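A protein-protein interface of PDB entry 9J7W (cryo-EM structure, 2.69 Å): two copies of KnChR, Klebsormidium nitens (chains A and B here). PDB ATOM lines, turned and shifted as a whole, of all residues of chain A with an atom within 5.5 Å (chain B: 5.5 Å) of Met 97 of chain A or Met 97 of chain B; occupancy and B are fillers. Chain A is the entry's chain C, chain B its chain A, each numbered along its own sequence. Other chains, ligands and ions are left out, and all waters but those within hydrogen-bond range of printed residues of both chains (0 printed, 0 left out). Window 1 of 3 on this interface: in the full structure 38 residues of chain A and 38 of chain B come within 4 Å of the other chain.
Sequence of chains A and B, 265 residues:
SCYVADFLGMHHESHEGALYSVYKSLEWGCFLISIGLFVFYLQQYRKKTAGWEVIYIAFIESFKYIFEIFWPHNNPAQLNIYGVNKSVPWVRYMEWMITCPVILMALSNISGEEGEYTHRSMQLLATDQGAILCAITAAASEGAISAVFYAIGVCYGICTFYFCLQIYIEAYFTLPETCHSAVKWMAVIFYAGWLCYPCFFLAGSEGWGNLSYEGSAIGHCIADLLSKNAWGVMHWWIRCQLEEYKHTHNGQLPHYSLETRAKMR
The side-chain amide nitrogen of Gln 129 of chain B is in hydrogen-bond range of the backbone carbonyl oxygen of Met 97 of chain A, 3.0 Å away. The side-chain amide oxygen of Gln 129 of chain B sits at hydrogen-bond distance from the side-chain amide nitrogen of Gln 129 of chain A (2.6 Å). The side-chain amide nitrogen (NE2) of Gln 129 of chain A lies within hydrogen-bond range of the backbone carbonyl oxygen (O) of Met 97 of chain B (3.0 Å).
Among the printed residues, pairs that only touch across the chains: Met 97 of chain A with Met 97 of chain B, Leu 133 of chain A with Ile 98 of chain B, Ile 98 of chain A with Leu 133 of chain B, Gln 129 of chain A with Pro 101 of chain B, Pro 101 of chain A with Gln 129 of chain B, Met 97 of chain A with Leu 133 of chain B, Leu 133 of chain A with Met 97 of chain B, Met 94 of chain A with Leu 133 of chain B and Leu 133 of chain A with Met 94 of chain B.
Met 97 of chain A touches just these residues of chain B: Met 97, Gln 129 and Leu 133. Of the printed residues of chain B, Gln 129 of chain A touches Met 97, Pro 101 and Gln 129. Ile 136 of chain A touches none of the printed residues of chain B. Printed residues of chain A within 4 Å of Met 94 of chain B: Leu 133 (3.9 Å). Printed residues of chain A within 4 Å of Met 97 of chain B: Met 97 (3.3 Å), Gln 129 (3.0 Å) and Leu 133 (3.7 Å). Of the printed residues of chain A, Leu 133 of chain B touches Met 94, Met 97 and Ile 98.
Of the 14 printed residues of chain B, 6 touch a printed residue of chain A. Printed residues of chain B that touch a printed residue of chain A: Met 94, Met 97, Ile 98, Pro 101, Gln 129 and Leu 133. Hydrophobic or aromatic side chains of chain B within 4 Å of the printed part of chain A: Met 94, Met 97, Ile 98, Pro 101 and Leu 133. Of the 14 printed residues of chain A, 6 touch a printed residue of chain B. Hydrophobic or aromatic side chains of chain A within 4 Å of the printed part of chain B: Met 94, Met 97, Ile 98, Pro 101 and Leu 133. Among the printed residues, no Asp or Glu carboxylate lies within 4 Å of a Lys or Arg side-chain nitrogen of the other chain.
Met 94 of chain A touches Leu 133 of chain B, and with the chains exchanged Leu 133 of chain A touches Met 94 of chain B. Met 97 of chain A touches its own counterpart, Met 97 of chain B. Met 97 of chain A touches Leu 133 of chain B, and with the chains exchanged Leu 133 of chain A touches Met 97 of chain B. Gln 129 of chain B touches its own counterpart, Gln 129 of chain A. 14 positions are printed for both chains.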
ATOM      1  N   ARG A  92     -16.629  12.365   0.503  1.00  0.00           N
ATOM      2  CA  ARG A  92     -17.419  11.333   1.169  1.00  0.00           C
ATOM      3  C   ARG A  92     -18.771  11.143   0.491  1.00  0.00           C
ATOM      4  O   ARG A  92     -19.202  10.011   0.238  1.00  0.00           O
ATOM      5  CB  ARG A  92     -17.599  11.705   2.644  1.00  0.00           C
ATOM      6  CG  ARG A  92     -18.564  10.828   3.417  1.00  0.00           C
ATOM      7  CD  ARG A  92     -18.812  11.367   4.808  1.00  0.00           C
ATOM      8  NE  ARG A  92     -17.588  11.472   5.591  1.00  0.00           N
ATOM      9  CZ  ARG A  92     -17.461  12.214   6.684  1.00  0.00           C
ATOM     10  NH1 ARG A  92     -18.454  12.962   7.131  1.00  0.00           N
ATOM     11  NH2 ARG A  92     -16.308  12.203   7.344  1.00  0.00           N
ATOM     12  N   TYR A  93     -19.456  12.242   0.177  1.00  0.00           N
ATOM     13  CA  TYR A  93     -20.801  12.137  -0.375  1.00  0.00           C
ATOM     14  C   TYR A  93     -20.767  11.680  -1.827  1.00  0.00           C
ATOM     15  O   TYR A  93     -21.656  10.953  -2.278  1.00  0.00           O
ATOM     16  CB  TYR A  93     -21.517  13.478  -0.235  1.00  0.00           C
ATOM     17  CG  TYR A  93     -21.700  13.916   1.201  1.00  0.00           C
ATOM     18  CD1 TYR A  93     -21.779  12.986   2.227  1.00  0.00           C
ATOM     19  CD2 TYR A  93     -21.780  15.258   1.534  1.00  0.00           C
ATOM     20  CE1 TYR A  93     -21.939  13.377   3.534  1.00  0.00           C
ATOM     21  CE2 TYR A  93     -21.939  15.657   2.843  1.00  0.00           C
ATOM     22  CZ  TYR A  93     -22.018  14.711   3.839  1.00  0.00           C
ATOM     23  OH  TYR A  93     -22.177  15.097   5.148  1.00  0.00           O
ATOM     24  N   MET A  94     -19.744  12.096  -2.574  1.00  0.00           N
ATOM     25  CA  MET A  94     -19.529  11.562  -3.913  1.00  0.00           C
ATOM     26  C   MET A  94     -19.320  10.056  -3.874  1.00  0.00           C
ATOM     27  O   MET A  94     -19.885   9.317  -4.691  1.00  0.00           O
ATOM     28  CB  MET A  94     -18.320  12.248  -4.542  1.00  0.00           C
ATOM     29  CG  MET A  94     -18.132  11.992  -6.025  1.00  0.00           C
ATOM     30  SD  MET A  94     -17.085  13.222  -6.811  1.00  0.00           S
ATOM     31  CE  MET A  94     -16.933  12.508  -8.440  1.00  0.00           C
ATOM     32  N   GLU A  95     -18.506   9.581  -2.931  1.00  0.00           N
ATOM     33  CA  GLU A  95     -18.292   8.148  -2.796  1.00  0.00           C
ATOM     34  C   GLU A  95     -19.585   7.434  -2.424  1.00  0.00           C
ATOM     35  O   GLU A  95     -19.860   6.343  -2.939  1.00  0.00           O
ATOM     36  CB  GLU A  95     -17.203   7.902  -1.755  1.00  0.00           C
ATOM     37  CG  GLU A  95     -16.709   6.478  -1.676  1.00  0.00           C
ATOM     38  CD  GLU A  95     -17.566   5.585  -0.824  1.00  0.00           C
ATOM     39  OE1 GLU A  95     -18.207   6.083   0.126  1.00  0.00           O
ATOM     40  OE2 GLU A  95     -17.598   4.376  -1.117  1.00  0.00           O
ATOM     41  N   TRP A  96     -20.382   8.029  -1.537  1.00  0.00           N
ATOM     42  CA  TRP A  96     -21.700   7.481  -1.232  1.00  0.00           C
ATOM     43  C   TRP A  96     -22.550   7.359  -2.488  1.00  0.00           C
ATOM     44  O   TRP A  96     -23.126   6.301  -2.760  1.00  0.00           O
ATOM     45  CB  TRP A  96     -22.419   8.366  -0.218  1.00  0.00           C
ATOM     46  CG  TRP A  96     -21.862   8.340   1.162  1.00  0.00           C
ATOM     47  CD1 TRP A  96     -20.721   7.727   1.580  1.00  0.00           C
ATOM     48  CD2 TRP A  96     -22.429   8.965   2.316  1.00  0.00           C
ATOM     49  NE1 TRP A  96     -20.541   7.930   2.926  1.00  0.00           N
ATOM     50  CE2 TRP A  96     -21.578   8.688   3.400  1.00  0.00           C
ATOM     51  CE3 TRP A  96     -23.575   9.732   2.536  1.00  0.00           C
ATOM     52  CZ2 TRP A  96     -21.838   9.151   4.684  1.00  0.00           C
ATOM     53  CZ3 TRP A  96     -23.830  10.189   3.810  1.00  0.00           C
ATOM     54  CH2 TRP A  96     -22.967   9.898   4.869  1.00  0.00           C
ATOM     55  N   MET A  97     -22.647   8.440  -3.261  1.00  0.00           N
ATOM     56  CA  MET A  97     -23.478   8.425  -4.458  1.00  0.00           C
ATOM     57  C   MET A  97     -23.007   7.368  -5.443  1.00  0.00           C
ATOM     58  O   MET A  97     -23.825   6.733  -6.117  1.00  0.00           O
ATOM     59  CB  MET A  97     -23.468   9.801  -5.119  1.00  0.00           C
ATOM     60  CG  MET A  97     -24.020  10.931  -4.255  1.00  0.00           C
ATOM     61  SD  MET A  97     -25.818  11.044  -4.133  1.00  0.00           S
ATOM     62  CE  MET A  97     -26.331  10.893  -5.831  1.00  0.00           C
ATOM     63  N   ILE A  98     -21.694   7.176  -5.558  1.00  0.00           N
ATOM     64  CA  ILE A  98     -21.181   6.152  -6.461  1.00  0.00           C
ATOM     65  C   ILE A  98     -21.521   4.755  -5.954  1.00  0.00           C
ATOM     66  O   ILE A  98     -22.012   3.913  -6.711  1.00  0.00           O
ATOM     67  CB  ILE A  98     -19.664   6.316  -6.652  1.00  0.00           C
ATOM     68  CG1 ILE A  98     -19.346   7.629  -7.364  1.00  0.00           C
ATOM     69  CG2 ILE A  98     -19.114   5.154  -7.450  1.00  0.00           C
ATOM     70  CD1 ILE A  98     -17.896   8.019  -7.289  1.00  0.00           C
ATOM     71  N   THR A  99     -21.277   4.485  -4.671  1.00  0.00           N
ATOM     72  CA  THR A  99     -21.304   3.115  -4.169  1.00  0.00           C
ATOM     73  C   THR A  99     -22.696   2.631  -3.783  1.00  0.00           C
ATOM     74  O   THR A  99     -23.062   1.500  -4.116  1.00  0.00           O
ATOM     75  CB  THR A  99     -20.368   2.977  -2.966  1.00  0.00           C
ATOM     76  OG1 THR A  99     -20.714   3.946  -1.969  1.00  0.00           O
ATOM     77  CG2 THR A  99     -18.920   3.157  -3.389  1.00  0.00           C
ATOM     78  N   CYS A 100     -23.475   3.449  -3.078  1.00  0.00           N
ATOM     79  CA  CYS A 100     -24.780   2.993  -2.606  1.00  0.00           C
ATOM     80  C   CYS A 100     -25.633   2.437  -3.735  1.00  0.00           C
ATOM     81  O   CYS A 100     -26.222   1.355  -3.563  1.00  0.00           O
ATOM     82  CB  CYS A 100     -25.481   4.147  -1.884  1.00  0.00           C
ATOM     83  SG  CYS A 100     -24.684   4.643  -0.352  1.00  0.00           S
ATOM     84  N   PRO A 101     -25.749   3.096  -4.891  1.00  0.00           N
ATOM     85  CA  PRO A 101     -26.452   2.458  -6.011  1.00  0.00           C
ATOM     86  C   PRO A 101     -25.853   1.123  -6.398  1.00  0.00           C
ATOM     87  O   PRO A 101     -26.593   0.174  -6.669  1.00  0.00           O
ATOM     88  CB  PRO A 101     -26.314   3.490  -7.137  1.00  0.00           C
ATOM     89  CG  PRO A 101     -26.085   4.770  -6.451  1.00  0.00           C
ATOM     90  CD  PRO A 101     -25.281   4.444  -5.248  1.00  0.00           C
ATOM     91  N   GLN A 129     -31.172   7.350  -4.464  1.00  0.00           N
ATOM     92  CA  GLN A 129     -30.687   8.585  -5.060  1.00  0.00           C
ATOM     93  C   GLN A 129     -31.260   9.797  -4.341  1.00  0.00           C
ATOM     94  O   GLN A 129     -30.519  10.707  -3.947  1.00  0.00           O
ATOM     95  CB  GLN A 129     -31.066   8.615  -6.537  1.00  0.00           C
ATOM     96  CG  GLN A 129     -30.344   9.656  -7.359  1.00  0.00           C
ATOM     97  CD  GLN A 129     -28.989   9.182  -7.822  1.00  0.00           C
ATOM     98  OE1 GLN A 129     -28.354   8.348  -7.178  1.00  0.00           O
ATOM     99  NE2 GLN A 129     -28.540   9.702  -8.952  1.00  0.00           N
ATOM    100  N   ILE A 132     -29.786  10.224  -0.696  1.00  0.00           N
ATOM    101  CA  ILE A 132     -28.431  10.754  -0.593  1.00  0.00           C
ATOM    102  C   ILE A 132     -28.371  12.199  -1.078  1.00  0.00           C
ATOM    103  O   ILE A 132     -27.641  13.020  -0.507  1.00  0.00           O
ATOM    104  CB  ILE A 132     -27.436   9.864  -1.355  1.00  0.00           C
ATOM    105  CG1 ILE A 132     -27.612   8.391  -0.971  1.00  0.00           C
ATOM    106  CG2 ILE A 132     -26.012  10.300  -1.073  1.00  0.00           C
ATOM    107  CD1 ILE A 132     -27.244   8.060   0.457  1.00  0.00           C
ATOM    108  N   LEU A 133     -29.122  12.543  -2.126  1.00  0.00           N
ATOM    109  CA  LEU A 133     -29.133  13.924  -2.593  1.00  0.00           C
ATOM    110  C   LEU A 133     -29.674  14.864  -1.524  1.00  0.00           C
ATOM    111  O   LEU A 133     -29.123  15.948  -1.303  1.00  0.00           O
ATOM    112  CB  LEU A 133     -29.966  14.030  -3.865  1.00  0.00           C
ATOM    113  CG  LEU A 133     -29.326  13.492  -5.141  1.00  0.00           C
ATOM    114  CD1 LEU A 133     -30.345  13.472  -6.253  1.00  0.00           C
ATOM    115  CD2 LEU A 133     -28.124  14.326  -5.534  1.00  0.00           C
ATOM    116  N   ILE A 136     -27.071  15.411   1.110  1.00  0.00           N
ATOM    117  CA  ILE A 136     -26.090  16.408   0.692  1.00  0.00           C
ATOM    118  C   ILE A 136     -26.665  17.812   0.827  1.00  0.00           C
ATOM    119  O   ILE A 136     -25.996  18.730   1.319  1.00  0.00           O
ATOM    120  CB  ILE A 136     -25.622  16.137  -0.747  1.00  0.00           C
ATOM    121  CG1 ILE A 136     -24.952  14.769  -0.852  1.00  0.00           C
ATOM    122  CG2 ILE A 136     -24.670  17.226  -1.208  1.00  0.00           C
ATOM    123  CD1 ILE A 136     -24.810  14.281  -2.265  1.00  0.00           C
ATOM    124  N   ARG B  92     -30.080  22.763 -10.112  1.00  0.00           N
ATOM    125  CA  ARG B  92     -30.003  22.185 -11.451  1.00  0.00           C
ATOM    126  C   ARG B  92     -29.347  20.808 -11.426  1.00  0.00           C
ATOM    127  O   ARG B  92     -29.840  19.857 -12.043  1.00  0.00           O
ATOM    128  CB  ARG B  92     -29.237  23.136 -12.373  1.00  0.00           C
ATOM    129  CG  ARG B  92     -28.908  22.581 -13.744  1.00  0.00           C
ATOM    130  CD  ARG B  92     -28.006  23.514 -14.521  1.00  0.00           C
ATOM    131  NE  ARG B  92     -28.599  24.831 -14.710  1.00  0.00           N
ATOM    132  CZ  ARG B  92     -27.915  25.918 -15.039  1.00  0.00           C
ATOM    133  NH1 ARG B  92     -26.602  25.891 -15.186  1.00  0.00           N
ATOM    134  NH2 ARG B  92     -28.566  27.062 -15.226  1.00  0.00           N
ATOM    135  N   TYR B  93     -28.231  20.679 -10.708  1.00  0.00           N
ATOM    136  CA  TYR B  93     -27.490  19.424 -10.723  1.00  0.00           C
ATOM    137  C   TYR B  93     -28.202  18.353  -9.909  1.00  0.00           C
ATOM    138  O   TYR B  93     -28.160  17.169 -10.256  1.00  0.00           O
ATOM    139  CB  TYR B  93     -26.074  19.661 -10.205  1.00  0.00           C
ATOM    140  CG  TYR B  93     -25.272  20.618 -11.059  1.00  0.00           C
ATOM    141  CD1 TYR B  93     -25.541  20.766 -12.411  1.00  0.00           C
ATOM    142  CD2 TYR B  93     -24.257  21.385 -10.510  1.00  0.00           C
ATOM    143  CE1 TYR B  93     -24.822  21.636 -13.191  1.00  0.00           C
ATOM    144  CE2 TYR B  93     -23.531  22.262 -11.286  1.00  0.00           C
ATOM    145  CZ  TYR B  93     -23.819  22.384 -12.628  1.00  0.00           C
ATOM    146  OH  TYR B  93     -23.101  23.255 -13.412  1.00  0.00           O
ATOM    147  N   MET B  94     -28.864  18.750  -8.823  1.00  0.00           N
ATOM    148  CA  MET B  94     -29.725  17.829  -8.091  1.00  0.00           C
ATOM    149  C   MET B  94     -30.838  17.297  -8.982  1.00  0.00           C
ATOM    150  O   MET B  94     -31.134  16.095  -8.974  1.00  0.00           O
ATOM    151  CB  MET B  94     -30.313  18.543  -6.878  1.00  0.00           C
ATOM    152  CG  MET B  94     -31.013  17.645  -5.877  1.00  0.00           C
ATOM    153  SD  MET B  94     -31.177  18.408  -4.261  1.00  0.00           S
ATOM    154  CE  MET B  94     -32.188  17.186  -3.438  1.00  0.00           C
ATOM    155  N   GLU B  95     -31.471  18.180  -9.754  1.00  0.00           N
ATOM    156  CA  GLU B  95     -32.514  17.744 -10.670  1.00  0.00           C
ATOM    157  C   GLU B  95     -31.954  16.805 -11.730  1.00  0.00           C
ATOM    158  O   GLU B  95     -32.603  15.814 -12.086  1.00  0.00           O
ATOM    159  CB  GLU B  95     -33.169  18.969 -11.301  1.00  0.00           C
ATOM    160  CG  GLU B  95     -34.421  18.684 -12.094  1.00  0.00           C
ATOM    161  CD  GLU B  95     -34.157  18.238 -13.505  1.00  0.00           C
ATOM    162  OE1 GLU B  95     -33.122  18.630 -14.083  1.00  0.00           O
ATOM    163  OE2 GLU B  95     -34.997  17.484 -14.031  1.00  0.00           O
ATOM    164  N   TRP B  96     -30.760  17.103 -12.245  1.00  0.00           N
ATOM    165  CA  TRP B  96     -30.094  16.184 -13.163  1.00  0.00           C
ATOM    166  C   TRP B  96     -29.905  14.814 -12.529  1.00  0.00           C
ATOM    167  O   TRP B  96     -30.253  13.789 -13.127  1.00  0.00           O
ATOM    168  CB  TRP B  96     -28.734  16.742 -13.575  1.00  0.00           C
ATOM    169  CG  TRP B  96     -28.776  17.931 -14.468  1.00  0.00           C
ATOM    170  CD1 TRP B  96     -29.873  18.643 -14.846  1.00  0.00           C
ATOM    171  CD2 TRP B  96     -27.656  18.553 -15.101  1.00  0.00           C
ATOM    172  NE1 TRP B  96     -29.506  19.671 -15.676  1.00  0.00           N
ATOM    173  CE2 TRP B  96     -28.147  19.637 -15.849  1.00  0.00           C
ATOM    174  CE3 TRP B  96     -26.283  18.298 -15.108  1.00  0.00           C
ATOM    175  CZ2 TRP B  96     -27.316  20.463 -16.594  1.00  0.00           C
ATOM    176  CZ3 TRP B  96     -25.461  19.118 -15.849  1.00  0.00           C
ATOM    177  CH2 TRP B  96     -25.978  20.188 -16.582  1.00  0.00           C
ATOM    178  N   MET B  97     -29.347  14.776 -11.321  1.00  0.00           N
ATOM    179  CA  MET B  97     -29.086  13.503 -10.662  1.00  0.00           C
ATOM    180  C   MET B  97     -30.373  12.722 -10.443  1.00  0.00           C
ATOM    181  O   MET B  97     -30.382  11.492 -10.549  1.00  0.00           O
ATOM    182  CB  MET B  97     -28.382  13.738  -9.329  1.00  0.00           C
ATOM    183  CG  MET B  97     -27.024  14.424  -9.432  1.00  0.00           C
ATOM    184  SD  MET B  97     -25.635  13.388  -9.941  1.00  0.00           S
ATOM    185  CE  MET B  97     -25.825  11.953  -8.906  1.00  0.00           C
ATOM    186  N   ILE B  98     -31.465  13.414 -10.119  1.00  0.00           N
ATOM    187  CA  ILE B  98     -32.737  12.726  -9.932  1.00  0.00           C
ATOM    188  C   ILE B  98     -33.261  12.175 -11.252  1.00  0.00           C
ATOM    189  O   ILE B  98     -33.660  11.009 -11.333  1.00  0.00           O
ATOM    190  CB  ILE B  98     -33.763  13.668  -9.280  1.00  0.00           C
ATOM    191  CG1 ILE B  98     -33.332  14.042  -7.863  1.00  0.00           C
ATOM    192  CG2 ILE B  98     -35.123  13.003  -9.243  1.00  0.00           C
ATOM    193  CD1 ILE B  98     -34.094  15.205  -7.290  1.00  0.00           C
ATOM    194  N   THR B  99     -33.262  12.989 -12.308  1.00  0.00           N
ATOM    195  CA  THR B  99     -33.995  12.649 -13.524  1.00  0.00           C
ATOM    196  C   THR B  99     -33.211  11.763 -14.481  1.00  0.00           C
ATOM    197  O   THR B  99     -33.771  10.802 -15.021  1.00  0.00           O
ATOM    198  CB  THR B  99     -34.426  13.924 -14.252  1.00  0.00           C
ATOM    199  OG1 THR B  99     -33.283  14.751 -14.499  1.00  0.00           O
ATOM    200  CG2 THR B  99     -35.456  14.687 -13.436  1.00  0.00           C
ATOM    201  N   CYS B 100     -31.936  12.062 -14.720  1.00  0.00           N
ATOM    202  CA  CYS B 100     -31.172  11.295 -15.702  1.00  0.00           C
ATOM    203  C   CYS B 100     -31.229   9.801 -15.429  1.00  0.00           C
ATOM    204  O   CYS B 100     -31.465   9.028 -16.376  1.00  0.00           O
ATOM    205  CB  CYS B 100     -29.732  11.811 -15.727  1.00  0.00           C
ATOM    206  SG  CYS B 100     -29.564  13.488 -16.352  1.00  0.00           S
ATOM    207  N   PRO B 101     -31.033   9.324 -14.197  1.00  0.00           N
ATOM    208  CA  PRO B 101     -31.247   7.894 -13.940  1.00  0.00           C
ATOM    209  C   PRO B 101     -32.642   7.434 -14.303  1.00  0.00           C
ATOM    210  O   PRO B 101     -32.802   6.355 -14.877  1.00  0.00           O
ATOM    211  CB  PRO B 101     -30.981   7.772 -12.434  1.00  0.00           C
ATOM    212  CG  PRO B 101     -30.131   8.925 -12.105  1.00  0.00           C
ATOM    213  CD  PRO B 101     -30.592  10.028 -12.984  1.00  0.00           C
ATOM    214  N   GLN B 129     -24.299   8.027 -13.389  1.00  0.00           N
ATOM    215  CA  GLN B 129     -24.006   8.545 -12.061  1.00  0.00           C
ATOM    216  C   GLN B 129     -22.620   9.167 -12.015  1.00  0.00           C
ATOM    217  O   GLN B 129     -22.453  10.305 -11.554  1.00  0.00           O
ATOM    218  CB  GLN B 129     -24.115   7.413 -11.043  1.00  0.00           C
ATOM    219  CG  GLN B 129     -24.179   7.858  -9.602  1.00  0.00           C
ATOM    220  CD  GLN B 129     -25.577   8.235  -9.180  1.00  0.00           C
ATOM    221  OE1 GLN B 129     -26.394   8.655  -9.997  1.00  0.00           O
ATOM    222  NE2 GLN B 129     -25.864   8.076  -7.900  1.00  0.00           N
ATOM    223  N   ILE B 132     -22.409  12.535 -14.076  1.00  0.00           N
ATOM    224  CA  ILE B 132     -23.004  13.719 -13.463  1.00  0.00           C
ATOM    225  C   ILE B 132     -22.244  14.126 -12.205  1.00  0.00           C
ATOM    226  O   ILE B 132     -22.078  15.323 -11.935  1.00  0.00           O
ATOM    227  CB  ILE B 132     -24.495  13.490 -13.169  1.00  0.00           C
ATOM    228  CG1 ILE B 132     -25.219  12.936 -14.400  1.00  0.00           C
ATOM    229  CG2 ILE B 132     -25.152  14.785 -12.729  1.00  0.00           C
ATOM    230  CD1 ILE B 132     -25.310  13.890 -15.566  1.00  0.00           C
ATOM    231  N   LEU B 133     -21.769  13.159 -11.417  1.00  0.00           N
ATOM    232  CA  LEU B 133     -20.992  13.501 -10.231  1.00  0.00           C
ATOM    233  C   LEU B 133     -19.710  14.234 -10.603  1.00  0.00           C
ATOM    234  O   LEU B 133     -19.341  15.222  -9.958  1.00  0.00           O
ATOM    235  CB  LEU B 133     -20.673  12.236  -9.443  1.00  0.00           C
ATOM    236  CG  LEU B 133     -21.824  11.627  -8.646  1.00  0.00           C
ATOM    237  CD1 LEU B 133     -21.411  10.281  -8.103  1.00  0.00           C
ATOM    238  CD2 LEU B 133     -22.247  12.548  -7.520  1.00  0.00           C
ATOM    239  N   ILE B 136     -20.501  17.773 -11.531  1.00  0.00           N
ATOM    240  CA  ILE B 136     -20.667  18.611 -10.346  1.00  0.00           C
ATOM    241  C   ILE B 136     -19.313  18.965  -9.747  1.00  0.00           C
ATOM    242  O   ILE B 136     -19.063  20.118  -9.375  1.00  0.00           O
ATOM    243  CB  ILE B 136     -21.565  17.912  -9.311  1.00  0.00           C
ATOM    244  CG1 ILE B 136     -22.956  17.655  -9.886  1.00  0.00           C
ATOM    245  CG2 ILE B 136     -21.664  18.747  -8.048  1.00  0.00           C
ATOM    246  CD1 ILE B 136     -23.755  16.663  -9.091  1.00  0.00           C
